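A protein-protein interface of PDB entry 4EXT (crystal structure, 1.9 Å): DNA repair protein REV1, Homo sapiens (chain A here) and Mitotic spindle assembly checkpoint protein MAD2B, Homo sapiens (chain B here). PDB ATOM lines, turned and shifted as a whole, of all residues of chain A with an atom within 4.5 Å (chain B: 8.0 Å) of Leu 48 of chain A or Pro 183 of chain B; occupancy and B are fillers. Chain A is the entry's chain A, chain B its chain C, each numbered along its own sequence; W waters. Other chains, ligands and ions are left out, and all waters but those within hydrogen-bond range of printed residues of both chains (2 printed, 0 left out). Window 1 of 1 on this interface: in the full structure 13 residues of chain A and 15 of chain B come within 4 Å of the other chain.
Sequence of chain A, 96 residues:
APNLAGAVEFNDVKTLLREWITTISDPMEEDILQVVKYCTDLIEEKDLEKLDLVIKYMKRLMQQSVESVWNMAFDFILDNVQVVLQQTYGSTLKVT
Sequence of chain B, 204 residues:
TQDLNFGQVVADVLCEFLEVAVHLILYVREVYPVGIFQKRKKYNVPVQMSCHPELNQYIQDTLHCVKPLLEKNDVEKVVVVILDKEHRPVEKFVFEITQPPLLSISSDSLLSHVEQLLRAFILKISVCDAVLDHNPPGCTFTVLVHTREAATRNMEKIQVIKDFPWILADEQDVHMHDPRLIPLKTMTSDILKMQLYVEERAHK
The side-chain amino group of Lys 46 of chain A lies within salt-bridge range of the side-chain carboxylate of Glu 96 of chain B.
OE1 of Gln 195 of chain B sits close to O of Lys 46 of chain A, 2.9 Å away.
N of Leu 48 of chain A sits at hydrogen-bond distance from OE1 of Gln 195 of chain B, at 3.1 Å.
OE1 of Glu 49 of chain A lies within salt-bridge range of NZ of Lys 185 of chain B, at 2.9 Å.
N of Thr 186 of chain B sits at hydrogen-bond distance from OE1 of Glu 49 of chain A.
OH of Tyr 89 of chain A is in hydrogen-bond range of OE2 of Glu 96 of chain B, at 3.2 Å.
OH of Tyr 89 of chain A lies within hydrogen-bond range of NE2 of Gln 195 of chain B (3.3 Å).
OD2 of Asp 47 of chain A is in salt-bridge range of NZ of Lys 50 of chain A (3.5 Å).
The side-chain carboxylate (OE2) of Glu 96 of chain B is in salt-bridge range of the side-chain amino group (NZ) of Lys 77 of chain B.
The backbone NH (N) of Val 94 of chain B sits at hydrogen-bond distance from the backbone carbonyl oxygen (O) of Tyr 197 of chain B.
OE1 of Glu 96 of chain B lies within hydrogen-bond range of NE2 of Gln 195 of chain B.
O of Lys 185 of chain B lies within hydrogen-bond range of N of Leu 196 of chain B, 2.7 Å away.
The side-chain hydroxyl (OG1) of Thr 186 of chain B lies within hydrogen-bond range of the side-chain amide oxygen (OE1) of Gln 195 of chain B.
O of Lys 46 of chain A touches CG2 of Thr 186 of chain B (3.9 Å).
Asp 47 of chain A touches Thr 186 of chain B.
OE1 of Gln 195 of chain B touches CA of Asp 47 of chain A, at 3.9 Å.
O of Leu 48 of chain A touches CG of Pro 183 of chain B (3.4 Å).
OG1 of Thr 186 of chain B touches N of Leu 48 of chain A, at 3.7 Å.
Asp 52 of chain A touches Pro 183 of chain B (OD1 to CD, 3.99 Å).
CD2 of Leu 85 of chain A touches CD1 of Leu 181 of chain B (3.9 Å).
OH of Tyr 197 of chain B touches CD1 of Tyr 89 of chain A, at 3.5 Å.
Leu 181 of chain B touches Leu 93 of chain A.
Pro 183 of chain B touches Leu 93 of chain A.
Of the printed residues of chain B, Leu 48 of chain A touches Pro 183 (3.4 Å), Thr 186 (3.7 Å) and Gln 195 (3.1 Å).
Of the printed residues of chain B, Glu 49 of chain A touches Lys 185 (2.9 Å) and Thr 186 (2.9 Å).
Of the printed residues of chain B, Leu 85 of chain A touches Leu 181 (3.9 Å).
Ile 182 of chain B touches none of the printed residues of chain A.
Printed residues of chain A within 4 Å of Glu 199 of chain B: Tyr 89.
The nearest printed residue of chain B that does not touch Leu 48 of chain A is Tyr 197 of chain B (4.002 Å).
The nearest printed residue of chain A that does not touch Pro 183 of chain B is Glu 49 of chain A (4.01 Å).
Of the 10 printed residues of chain A, 8 touch a printed residue of chain B.
Hydrophobic or aromatic side chains of chain A that line the printed part of chain B: Leu 48, Leu 85, Tyr 89 and Leu 93.
Among the printed residues, 19 pairs touch across the chains.
Among the printed residues, Asp or Glu carboxylates within 4 Å of a Lys or Arg side-chain nitrogen of the other chain: Lys 46 of chain A with Glu 96 of chain B (3.7 Å) and Glu 49 of chain A with Lys 185 of chain B (2.9 Å).
Water W1 bridges OE1 of Glu 199 of chain B (2.8 Å) and O of Tyr 89 of chain A (3.4 Å).
Water W2 lies within hydrogen-bond range of OG1 of Thr 186 of chain B (2.9 Å), O of Leu 196 of chain B (3.2 Å), O of Lys 185 of chain B (3.2 Å) and N of Glu 49 of chain A (3.5 Å).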
ATOM      1  N   LYS A  46     -29.535  -2.077  -3.928  1.00  0.00           N
ATOM      2  CA  LYS A  46     -29.401  -3.381  -3.290  1.00  0.00           C
ATOM      3  C   LYS A  46     -29.006  -4.538  -4.205  1.00  0.00           C
ATOM      4  O   LYS A  46     -29.559  -5.633  -4.106  1.00  0.00           O
ATOM      5  CB  LYS A  46     -30.698  -3.714  -2.543  1.00  0.00           C
ATOM      6  CG  LYS A  46     -30.780  -3.016  -1.191  1.00  0.00           C
ATOM      7  CD  LYS A  46     -32.204  -2.841  -0.689  1.00  0.00           C
ATOM      8  CE  LYS A  46     -32.219  -2.576   0.817  1.00  0.00           C
ATOM      9  NZ  LYS A  46     -31.140  -1.625   1.256  1.00  0.00           N
ATOM     10  N   ASP A  47     -28.057  -4.300  -5.105  1.00  0.00           N
ATOM     11  CA  ASP A  47     -27.582  -5.372  -5.975  1.00  0.00           C
ATOM     12  C   ASP A  47     -26.091  -5.533  -5.706  1.00  0.00           C
ATOM     13  O   ASP A  47     -25.251  -5.152  -6.519  1.00  0.00           O
ATOM     14  CB  ASP A  47     -27.803  -5.049  -7.450  1.00  0.00           C
ATOM     15  CG  ASP A  47     -27.595  -6.267  -8.345  1.00  0.00           C
ATOM     16  OD1 ASP A  47     -26.987  -7.263  -7.879  1.00  0.00           O
ATOM     17  OD2 ASP A  47     -28.036  -6.224  -9.516  1.00  0.00           O
ATOM     18  N   LEU A  48     -25.775  -6.097  -4.549  1.00  0.00           N
ATOM     19  CA  LEU A  48     -24.397  -6.290  -4.153  1.00  0.00           C
ATOM     20  C   LEU A  48     -23.673  -7.369  -4.959  1.00  0.00           C
ATOM     21  O   LEU A  48     -22.445  -7.370  -5.021  1.00  0.00           O
ATOM     22  CB  LEU A  48     -24.334  -6.617  -2.663  1.00  0.00           C
ATOM     23  CG  LEU A  48     -24.805  -5.491  -1.734  1.00  0.00           C
ATOM     24  CD1 LEU A  48     -24.818  -5.998  -0.304  1.00  0.00           C
ATOM     25  CD2 LEU A  48     -23.879  -4.275  -1.884  1.00  0.00           C
ATOM     26  N   GLU A  49     -24.411  -8.291  -5.577  1.00  0.00           N
ATOM     27  CA  GLU A  49     -23.719  -9.318  -6.356  1.00  0.00           C
ATOM     28  C   GLU A  49     -23.096  -8.667  -7.578  1.00  0.00           C
ATOM     29  O   GLU A  49     -21.966  -8.954  -7.941  1.00  0.00           O
ATOM     30  CB  GLU A  49     -24.673 -10.428  -6.819  1.00  0.00           C
ATOM     31  CG  GLU A  49     -23.924 -11.638  -7.339  1.00  0.00           C
ATOM     32  CD  GLU A  49     -24.788 -12.559  -8.184  1.00  0.00           C
ATOM     33  OE1 GLU A  49     -26.027 -12.479  -8.086  1.00  0.00           O
ATOM     34  OE2 GLU A  49     -24.215 -13.363  -8.950  1.00  0.00           O
ATOM     35  N   LYS A  50     -23.855  -7.795  -8.221  1.00  0.00           N
ATOM     36  CA  LYS A  50     -23.373  -7.099  -9.403  1.00  0.00           C
ATOM     37  C   LYS A  50     -22.196  -6.190  -9.043  1.00  0.00           C
ATOM     38  O   LYS A  50     -21.242  -6.083  -9.800  1.00  0.00           O
ATOM     39  CB  LYS A  50     -24.513  -6.286 -10.024  1.00  0.00           C
ATOM     40  CG  LYS A  50     -24.222  -5.763 -11.415  1.00  0.00           C
ATOM     41  CD  LYS A  50     -25.482  -5.281 -12.085  1.00  0.00           C
ATOM     42  CE  LYS A  50     -26.402  -6.444 -12.416  1.00  0.00           C
ATOM     43  NZ  LYS A  50     -27.640  -5.941 -13.025  1.00  0.00           N
ATOM     44  N   LEU A  51     -22.267  -5.536  -7.884  1.00  0.00           N
ATOM     45  CA  LEU A  51     -21.180  -4.659  -7.449  1.00  0.00           C
ATOM     46  C   LEU A  51     -19.889  -5.453  -7.271  1.00  0.00           C
ATOM     47  O   LEU A  51     -18.821  -5.023  -7.709  1.00  0.00           O
ATOM     48  CB  LEU A  51     -21.541  -3.972  -6.126  1.00  0.00           C
ATOM     49  CG  LEU A  51     -20.399  -3.203  -5.446  1.00  0.00           C
ATOM     50  CD1 LEU A  51     -20.114  -1.921  -6.226  1.00  0.00           C
ATOM     51  CD2 LEU A  51     -20.776  -2.888  -3.996  1.00  0.00           C
ATOM     52  N   ASP A  52     -19.993  -6.614  -6.631  1.00  0.00           N
ATOM     53  CA  ASP A  52     -18.841  -7.480  -6.381  1.00  0.00           C
ATOM     54  C   ASP A  52     -18.191  -7.985  -7.672  1.00  0.00           C
ATOM     55  O   ASP A  52     -16.972  -7.971  -7.794  1.00  0.00           O
ATOM     56  CB  ASP A  52     -19.256  -8.678  -5.515  1.00  0.00           C
ATOM     57  CG  ASP A  52     -18.067  -9.536  -5.068  1.00  0.00           C
ATOM     58  OD1 ASP A  52     -17.211  -9.033  -4.308  1.00  0.00           O
ATOM     59  OD2 ASP A  52     -17.990 -10.719  -5.469  1.00  0.00           O
ATOM     60  N   LEU A  85     -20.151   1.858   1.300  1.00  0.00           N
ATOM     61  CA  LEU A  85     -20.599   0.590   1.891  1.00  0.00           C
ATOM     62  C   LEU A  85     -20.511   0.637   3.415  1.00  0.00           C
ATOM     63  O   LEU A  85     -21.398   0.165   4.129  1.00  0.00           O
ATOM     64  CB  LEU A  85     -19.732  -0.565   1.392  1.00  0.00           C
ATOM     65  CG  LEU A  85     -20.136  -1.187   0.062  1.00  0.00           C
ATOM     66  CD1 LEU A  85     -19.087  -2.209  -0.350  1.00  0.00           C
ATOM     67  CD2 LEU A  85     -21.517  -1.830   0.199  1.00  0.00           C
ATOM     68  N   TYR A  89     -24.000  -0.277   4.724  1.00  0.00           N
ATOM     69  CA  TYR A  89     -24.097  -1.660   5.183  1.00  0.00           C
ATOM     70  C   TYR A  89     -23.297  -1.887   6.457  1.00  0.00           C
ATOM     71  O   TYR A  89     -23.537  -2.850   7.187  1.00  0.00           O
ATOM     72  CB  TYR A  89     -23.631  -2.612   4.073  1.00  0.00           C
ATOM     73  CG  TYR A  89     -24.729  -2.932   3.088  1.00  0.00           C
ATOM     74  CD1 TYR A  89     -25.636  -3.961   3.348  1.00  0.00           C
ATOM     75  CD2 TYR A  89     -24.924  -2.159   1.949  1.00  0.00           C
ATOM     76  CE1 TYR A  89     -26.712  -4.210   2.509  1.00  0.00           C
ATOM     77  CE2 TYR A  89     -26.017  -2.399   1.095  1.00  0.00           C
ATOM     78  CZ  TYR A  89     -26.903  -3.428   1.392  1.00  0.00           C
ATOM     79  OH  TYR A  89     -27.998  -3.671   0.597  1.00  0.00           O
ATOM     80  N   LEU A  93     -16.336  -4.082   1.312  1.00  0.00           N
ATOM     81  CA  LEU A  93     -16.223  -5.189   0.394  1.00  0.00           C
ATOM     82  C   LEU A  93     -14.893  -5.908   0.548  1.00  0.00           C
ATOM     83  O   LEU A  93     -13.831  -5.281   0.603  1.00  0.00           O
ATOM     84  CB  LEU A  93     -16.380  -4.672  -1.035  1.00  0.00           C
ATOM     85  CG  LEU A  93     -16.679  -5.692  -2.126  1.00  0.00           C
ATOM     86  CD1 LEU A  93     -17.929  -6.500  -1.762  1.00  0.00           C
ATOM     87  CD2 LEU A  93     -16.885  -4.949  -3.449  1.00  0.00           C
ATOM     88  N   LYS B  77     -34.556  -8.461   7.034  1.00  0.00           N
ATOM     89  CA  LYS B  77     -33.438  -9.395   6.942  1.00  0.00           C
ATOM     90  C   LYS B  77     -33.574 -10.587   7.872  1.00  0.00           C
ATOM     91  O   LYS B  77     -34.072 -10.462   8.988  1.00  0.00           O
ATOM     92  CB  LYS B  77     -32.116  -8.715   7.319  1.00  0.00           C
ATOM     93  CG  LYS B  77     -31.755  -7.442   6.586  1.00  0.00           C
ATOM     94  CD  LYS B  77     -30.464  -6.871   7.177  1.00  0.00           C
ATOM     95  CE  LYS B  77     -30.075  -5.543   6.534  1.00  0.00           C
ATOM     96  NZ  LYS B  77     -29.677  -5.707   5.106  1.00  0.00           N
ATOM     97  N   VAL B  94     -26.521 -13.248   5.698  1.00  0.00           N
ATOM     98  CA  VAL B  94     -27.637 -12.327   5.644  1.00  0.00           C
ATOM     99  C   VAL B  94     -28.541 -12.476   4.441  1.00  0.00           C
ATOM    100  O   VAL B  94     -28.091 -12.379   3.299  1.00  0.00           O
ATOM    101  CB  VAL B  94     -27.124 -10.867   5.641  1.00  0.00           C
ATOM    102  CG1 VAL B  94     -28.294  -9.906   5.557  1.00  0.00           C
ATOM    103  CG2 VAL B  94     -26.276 -10.602   6.888  1.00  0.00           C
ATOM    104  N   GLU B  96     -31.291 -10.572   2.772  1.00  0.00           N
ATOM    105  CA  GLU B  96     -32.004  -9.298   2.714  1.00  0.00           C
ATOM    106  C   GLU B  96     -33.175  -9.550   1.778  1.00  0.00           C
ATOM    107  O   GLU B  96     -32.979  -9.861   0.599  1.00  0.00           O
ATOM    108  CB  GLU B  96     -31.094  -8.211   2.153  1.00  0.00           C
ATOM    109  CG  GLU B  96     -31.582  -6.799   2.401  1.00  0.00           C
ATOM    110  CD  GLU B  96     -30.642  -5.758   1.821  1.00  0.00           C
ATOM    111  OE1 GLU B  96     -30.427  -5.772   0.592  1.00  0.00           O
ATOM    112  OE2 GLU B  96     -30.117  -4.930   2.591  1.00  0.00           O
ATOM    113  N   LYS B 124     -24.566 -21.339  -4.439  1.00  0.00           N
ATOM    114  CA  LYS B 124     -23.563 -20.405  -3.940  1.00  0.00           C
ATOM    115  C   LYS B 124     -23.140 -20.759  -2.518  1.00  0.00           C
ATOM    116  O   LYS B 124     -21.966 -20.661  -2.166  1.00  0.00           O
ATOM    117  CB  LYS B 124     -24.106 -18.974  -3.996  1.00  0.00           C
ATOM    118  CG  LYS B 124     -23.890 -18.278  -5.341  1.00  0.00           C
ATOM    119  CD  LYS B 124     -22.393 -18.150  -5.630  1.00  0.00           C
ATOM    120  CE  LYS B 124     -22.103 -17.205  -6.790  1.00  0.00           C
ATOM    121  NZ  LYS B 124     -22.573 -17.743  -8.096  1.00  0.00           N
ATOM    122  N   CYS B 128     -19.401 -21.499  -0.967  1.00  0.00           N
ATOM    123  CA  CYS B 128     -18.939 -20.294  -0.275  1.00  0.00           C
ATOM    124  C   CYS B 128     -17.695 -20.568   0.568  1.00  0.00           C
ATOM    125  O   CYS B 128     -16.930 -19.652   0.893  1.00  0.00           O
ATOM    126  CB  CYS B 128     -20.050 -19.710   0.609  1.00  0.00           C
ATOM    127  SG  CYS B 128     -20.303 -20.572   2.166  1.00  0.00           S
ATOM    128  N   VAL B 131     -14.726 -18.639  -0.829  1.00  0.00           N
ATOM    129  CA  VAL B 131     -14.667 -17.188  -0.694  1.00  0.00           C
ATOM    130  C   VAL B 131     -14.609 -16.692   0.750  1.00  0.00           C
ATOM    131  O   VAL B 131     -14.568 -15.486   0.990  1.00  0.00           O
ATOM    132  CB  VAL B 131     -15.869 -16.515  -1.394  1.00  0.00           C
ATOM    133  CG1 VAL B 131     -15.815 -16.781  -2.889  1.00  0.00           C
ATOM    134  CG2 VAL B 131     -17.172 -17.033  -0.811  1.00  0.00           C
ATOM    135  N   LEU B 132     -14.593 -17.615   1.707  1.00  0.00           N
ATOM    136  CA  LEU B 132     -14.546 -17.246   3.121  1.00  0.00           C
ATOM    137  C   LEU B 132     -13.295 -17.783   3.816  1.00  0.00           C
ATOM    138  O   LEU B 132     -12.634 -18.684   3.307  1.00  0.00           O
ATOM    139  CB  LEU B 132     -15.795 -17.775   3.841  1.00  0.00           C
ATOM    140  CG  LEU B 132     -17.143 -17.321   3.268  1.00  0.00           C
ATOM    141  CD1 LEU B 132     -18.277 -18.064   3.943  1.00  0.00           C
ATOM    142  CD2 LEU B 132     -17.291 -15.821   3.445  1.00  0.00           C
ATOM    143  N   ARG B 180     -16.193  -7.734   6.983  1.00  0.00           N
ATOM    144  CA  ARG B 180     -15.901  -7.625   5.565  1.00  0.00           C
ATOM    145  C   ARG B 180     -17.096  -8.249   4.841  1.00  0.00           C
ATOM    146  O   ARG B 180     -17.628  -9.274   5.268  1.00  0.00           O
ATOM    147  CB  ARG B 180     -14.601  -8.353   5.220  1.00  0.00           C
ATOM    148  CG  ARG B 180     -13.376  -7.830   5.968  1.00  0.00           C
ATOM    149  CD  ARG B 180     -13.234  -6.315   5.822  1.00  0.00           C
ATOM    150  NE  ARG B 180     -12.095  -5.798   6.577  1.00  0.00           N
ATOM    151  CZ  ARG B 180     -10.828  -6.120   6.332  1.00  0.00           C
ATOM    152  NH1 ARG B 180     -10.534  -6.960   5.346  1.00  0.00           N
ATOM    153  NH2 ARG B 180      -9.855  -5.609   7.074  1.00  0.00           N
ATOM    154  N   LEU B 181     -17.526  -7.607   3.764  1.00  0.00           N
ATOM    155  CA  LEU B 181     -18.684  -8.037   2.992  1.00  0.00           C
ATOM    156  C   LEU B 181     -18.323  -8.988   1.854  1.00  0.00           C
ATOM    157  O   LEU B 181     -17.337  -8.772   1.146  1.00  0.00           O
ATOM    158  CB  LEU B 181     -19.382  -6.805   2.412  1.00  0.00           C
ATOM    159  CG  LEU B 181     -20.890  -6.618   2.572  1.00  0.00           C
ATOM    160  CD1 LEU B 181     -21.312  -5.341   1.841  1.00  0.00           C
ATOM    161  CD2 LEU B 181     -21.628  -7.819   2.009  1.00  0.00           C
ATOM    162  N   ILE B 182     -19.139 -10.028   1.676  1.00  0.00           N
ATOM    163  CA  ILE B 182     -18.929 -11.021   0.624  1.00  0.00           C
ATOM    164  C   ILE B 182     -20.293 -11.398   0.030  1.00  0.00           C
ATOM    165  O   ILE B 182     -20.992 -12.263   0.548  1.00  0.00           O
ATOM    166  CB  ILE B 182     -18.244 -12.277   1.199  1.00  0.00           C
ATOM    167  CG1 ILE B 182     -16.904 -11.876   1.814  1.00  0.00           C
ATOM    168  CG2 ILE B 182     -18.045 -13.323   0.108  1.00  0.00           C
ATOM    169  CD1 ILE B 182     -16.480 -12.741   2.957  1.00  0.00           C
ATOM    170  N   PRO B 183     -20.705 -10.707  -1.039  1.00  0.00           N
ATOM    171  CA  PRO B 183     -21.992 -10.999  -1.674  1.00  0.00           C
ATOM    172  C   PRO B 183     -21.933 -12.384  -2.288  1.00  0.00           C
ATOM    173  O   PRO B 183     -20.891 -12.797  -2.784  1.00  0.00           O
ATOM    174  CB  PRO B 183     -22.104  -9.908  -2.725  1.00  0.00           C
ATOM    175  CG  PRO B 183     -21.320  -8.770  -2.103  1.00  0.00           C
ATOM    176  CD  PRO B 183     -20.110  -9.486  -1.607  1.00  0.00           C
ATOM    177  N   LEU B 184     -23.041 -13.109  -2.238  1.00  0.00           N
ATOM    178  CA  LEU B 184     -23.074 -14.447  -2.799  1.00  0.00           C
ATOM    179  C   LEU B 184     -24.053 -14.483  -3.959  1.00  0.00           C
ATOM    180  O   LEU B 184     -23.727 -14.978  -5.032  1.00  0.00           O
ATOM    181  CB  LEU B 184     -23.489 -15.462  -1.734  1.00  0.00           C
ATOM    182  CG  LEU B 184     -22.543 -15.683  -0.551  1.00  0.00           C
ATOM    183  CD1 LEU B 184     -23.070 -16.824   0.308  1.00  0.00           C
ATOM    184  CD2 LEU B 184     -21.141 -16.012  -1.056  1.00  0.00           C
ATOM    185  N   LYS B 185     -25.248 -13.941  -3.746  1.00  0.00           N
ATOM    186  CA  LYS B 185     -26.248 -13.936  -4.796  1.00  0.00           C
ATOM    187  C   LYS B 185     -27.339 -12.906  -4.602  1.00  0.00           C
ATOM    188  O   LYS B 185     -27.809 -12.685  -3.491  1.00  0.00           O
ATOM    189  CB  LYS B 185     -26.898 -15.320  -4.908  1.00  0.00           C
ATOM    190  CG  LYS B 185     -27.801 -15.451  -6.108  1.00  0.00           C
ATOM    191  CD  LYS B 185     -26.989 -15.352  -7.382  1.00  0.00           C
ATOM    192  CE  LYS B 185     -27.818 -14.798  -8.521  1.00  0.00           C
ATOM    193  NZ  LYS B 185     -26.992 -14.649  -9.744  1.00  0.00           N
ATOM    194  N   THR B 186     -27.747 -12.290  -5.705  1.00  0.00           N
ATOM    195  CA  THR B 186     -28.817 -11.303  -5.709  1.00  0.00           C
ATOM    196  C   THR B 186     -29.819 -11.720  -6.786  1.00  0.00           C
ATOM    197  O   THR B 186     -29.440 -11.946  -7.937  1.00  0.00           O
ATOM    198  CB  THR B 186     -28.295  -9.894  -6.080  1.00  0.00           C
ATOM    199  OG1 THR B 186     -27.370  -9.435  -5.082  1.00  0.00           O
ATOM    200  CG2 THR B 186     -29.452  -8.914  -6.199  1.00  0.00           C
ATOM    201  N   LYS B 193     -37.690 -10.099  -4.372  1.00  0.00           N
ATOM    202  CA  LYS B 193     -36.395  -9.470  -4.619  1.00  0.00           C
ATOM    203  C   LYS B 193     -35.574  -9.784  -3.366  1.00  0.00           C
ATOM    204  O   LYS B 193     -35.925  -9.357  -2.266  1.00  0.00           O
ATOM    205  CB  LYS B 193     -36.593  -7.963  -4.785  1.00  0.00           C
ATOM    206  CG  LYS B 193     -35.475  -7.209  -5.497  1.00  0.00           C
ATOM    207  CD  LYS B 193     -34.258  -6.989  -4.610  1.00  0.00           C
ATOM    208  CE  LYS B 193     -33.352  -5.885  -5.178  1.00  0.00           C
ATOM    209  NZ  LYS B 193     -32.871  -6.163  -6.567  1.00  0.00           N
ATOM    210  N   GLN B 195     -31.411 -10.908  -1.678  1.00  0.00           N
ATOM    211  CA  GLN B 195     -29.967 -11.112  -1.671  1.00  0.00           C
ATOM    212  C   GLN B 195     -29.304 -11.758  -0.546  1.00  0.00           C
ATOM    213  O   GLN B 195     -29.723 -11.588   0.502  1.00  0.00           O
ATOM    214  CB  GLN B 195     -29.222  -9.914  -2.006  1.00  0.00           C
ATOM    215  CG  GLN B 195     -29.219  -8.739  -1.200  1.00  0.00           C
ATOM    216  CD  GLN B 195     -28.473  -7.496  -1.785  1.00  0.00           C
ATOM    217  OE1 GLN B 195     -27.873  -7.527  -2.782  1.00  0.00           O
ATOM    218  NE2 GLN B 195     -28.530  -6.448  -1.080  1.00  0.00           N
ATOM    219  N   LEU B 196     -28.296 -12.504  -0.865  1.00  0.00           N
ATOM    220  CA  LEU B 196     -27.587 -13.204   0.169  1.00  0.00           C
ATOM    221  C   LEU B 196     -26.148 -12.744   0.143  1.00  0.00           C
ATOM    222  O   LEU B 196     -25.497 -12.765  -0.905  1.00  0.00           O
ATOM    223  CB  LEU B 196     -27.658 -14.716  -0.085  1.00  0.00           C
ATOM    224  CG  LEU B 196     -26.689 -15.633   0.666  1.00  0.00           C
ATOM    225  CD1 LEU B 196     -26.920 -15.538   2.154  1.00  0.00           C
ATOM    226  CD2 LEU B 196     -26.870 -17.066   0.194  1.00  0.00           C
ATOM    227  N   TYR B 197     -25.672 -12.279   1.288  1.00  0.00           N
ATOM    228  CA  TYR B 197     -24.286 -11.863   1.420  1.00  0.00           C
ATOM    229  C   TYR B 197     -23.808 -12.286   2.789  1.00  0.00           C
ATOM    230  O   TYR B 197     -24.611 -12.495   3.690  1.00  0.00           O
ATOM    231  CB  TYR B 197     -24.108 -10.345   1.244  1.00  0.00           C
ATOM    232  CG  TYR B 197     -24.841  -9.468   2.239  1.00  0.00           C
ATOM    233  CD1 TYR B 197     -26.130  -9.015   1.975  1.00  0.00           C
ATOM    234  CD2 TYR B 197     -24.229  -9.060   3.428  1.00  0.00           C
ATOM    235  CE1 TYR B 197     -26.800  -8.169   2.879  1.00  0.00           C
ATOM    236  CE2 TYR B 197     -24.890  -8.207   4.334  1.00  0.00           C
ATOM    237  CZ  TYR B 197     -26.172  -7.770   4.046  1.00  0.00           C
ATOM    238  OH  TYR B 197     -26.828  -6.917   4.907  1.00  0.00           O
ATOM    239  N   VAL B 198     -22.494 -12.427   2.937  1.00  0.00           N
ATOM    240  CA  VAL B 198     -21.907 -12.824   4.205  1.00  0.00           C
ATOM    241  C   VAL B 198     -21.076 -11.678   4.777  1.00  0.00           C
ATOM    242  O   VAL B 198     -20.397 -10.962   4.038  1.00  0.00           O
ATOM    243  CB  VAL B 198     -20.976 -14.057   4.035  1.00  0.00           C
ATOM    244  CG1 VAL B 198     -20.393 -14.467   5.382  1.00  0.00           C
ATOM    245  CG2 VAL B 198     -21.743 -15.216   3.416  1.00  0.00           C
ATOM    246  N   GLU B 199     -21.188 -11.474   6.083  1.00  0.00           N
ATOM    247  CA  GLU B 199     -20.388 -10.470   6.773  1.00  0.00           C
ATOM    248  C   GLU B 199     -19.409 -11.333   7.544  1.00  0.00           C
ATOM    249  O   GLU B 199     -19.811 -12.201   8.323  1.00  0.00           O
ATOM    250  CB  GLU B 199     -21.221  -9.637   7.734  1.00  0.00           C
ATOM    251  CG  GLU B 199     -22.268  -8.802   7.049  1.00  0.00           C
ATOM    252  CD  GLU B 199     -22.576  -7.536   7.812  1.00  0.00           C
ATOM    253  OE1 GLU B 199     -22.881  -7.631   9.024  1.00  0.00           O
ATOM    254  OE2 GLU B 199     -22.513  -6.451   7.191  1.00  0.00           O
HETATM  255  O   HOH W   1     -22.476  -4.914   9.671  1.00  0.00           O
HETATM  256  O   HOH W   2     -25.595 -10.406  -3.058  1.00  0.00           O
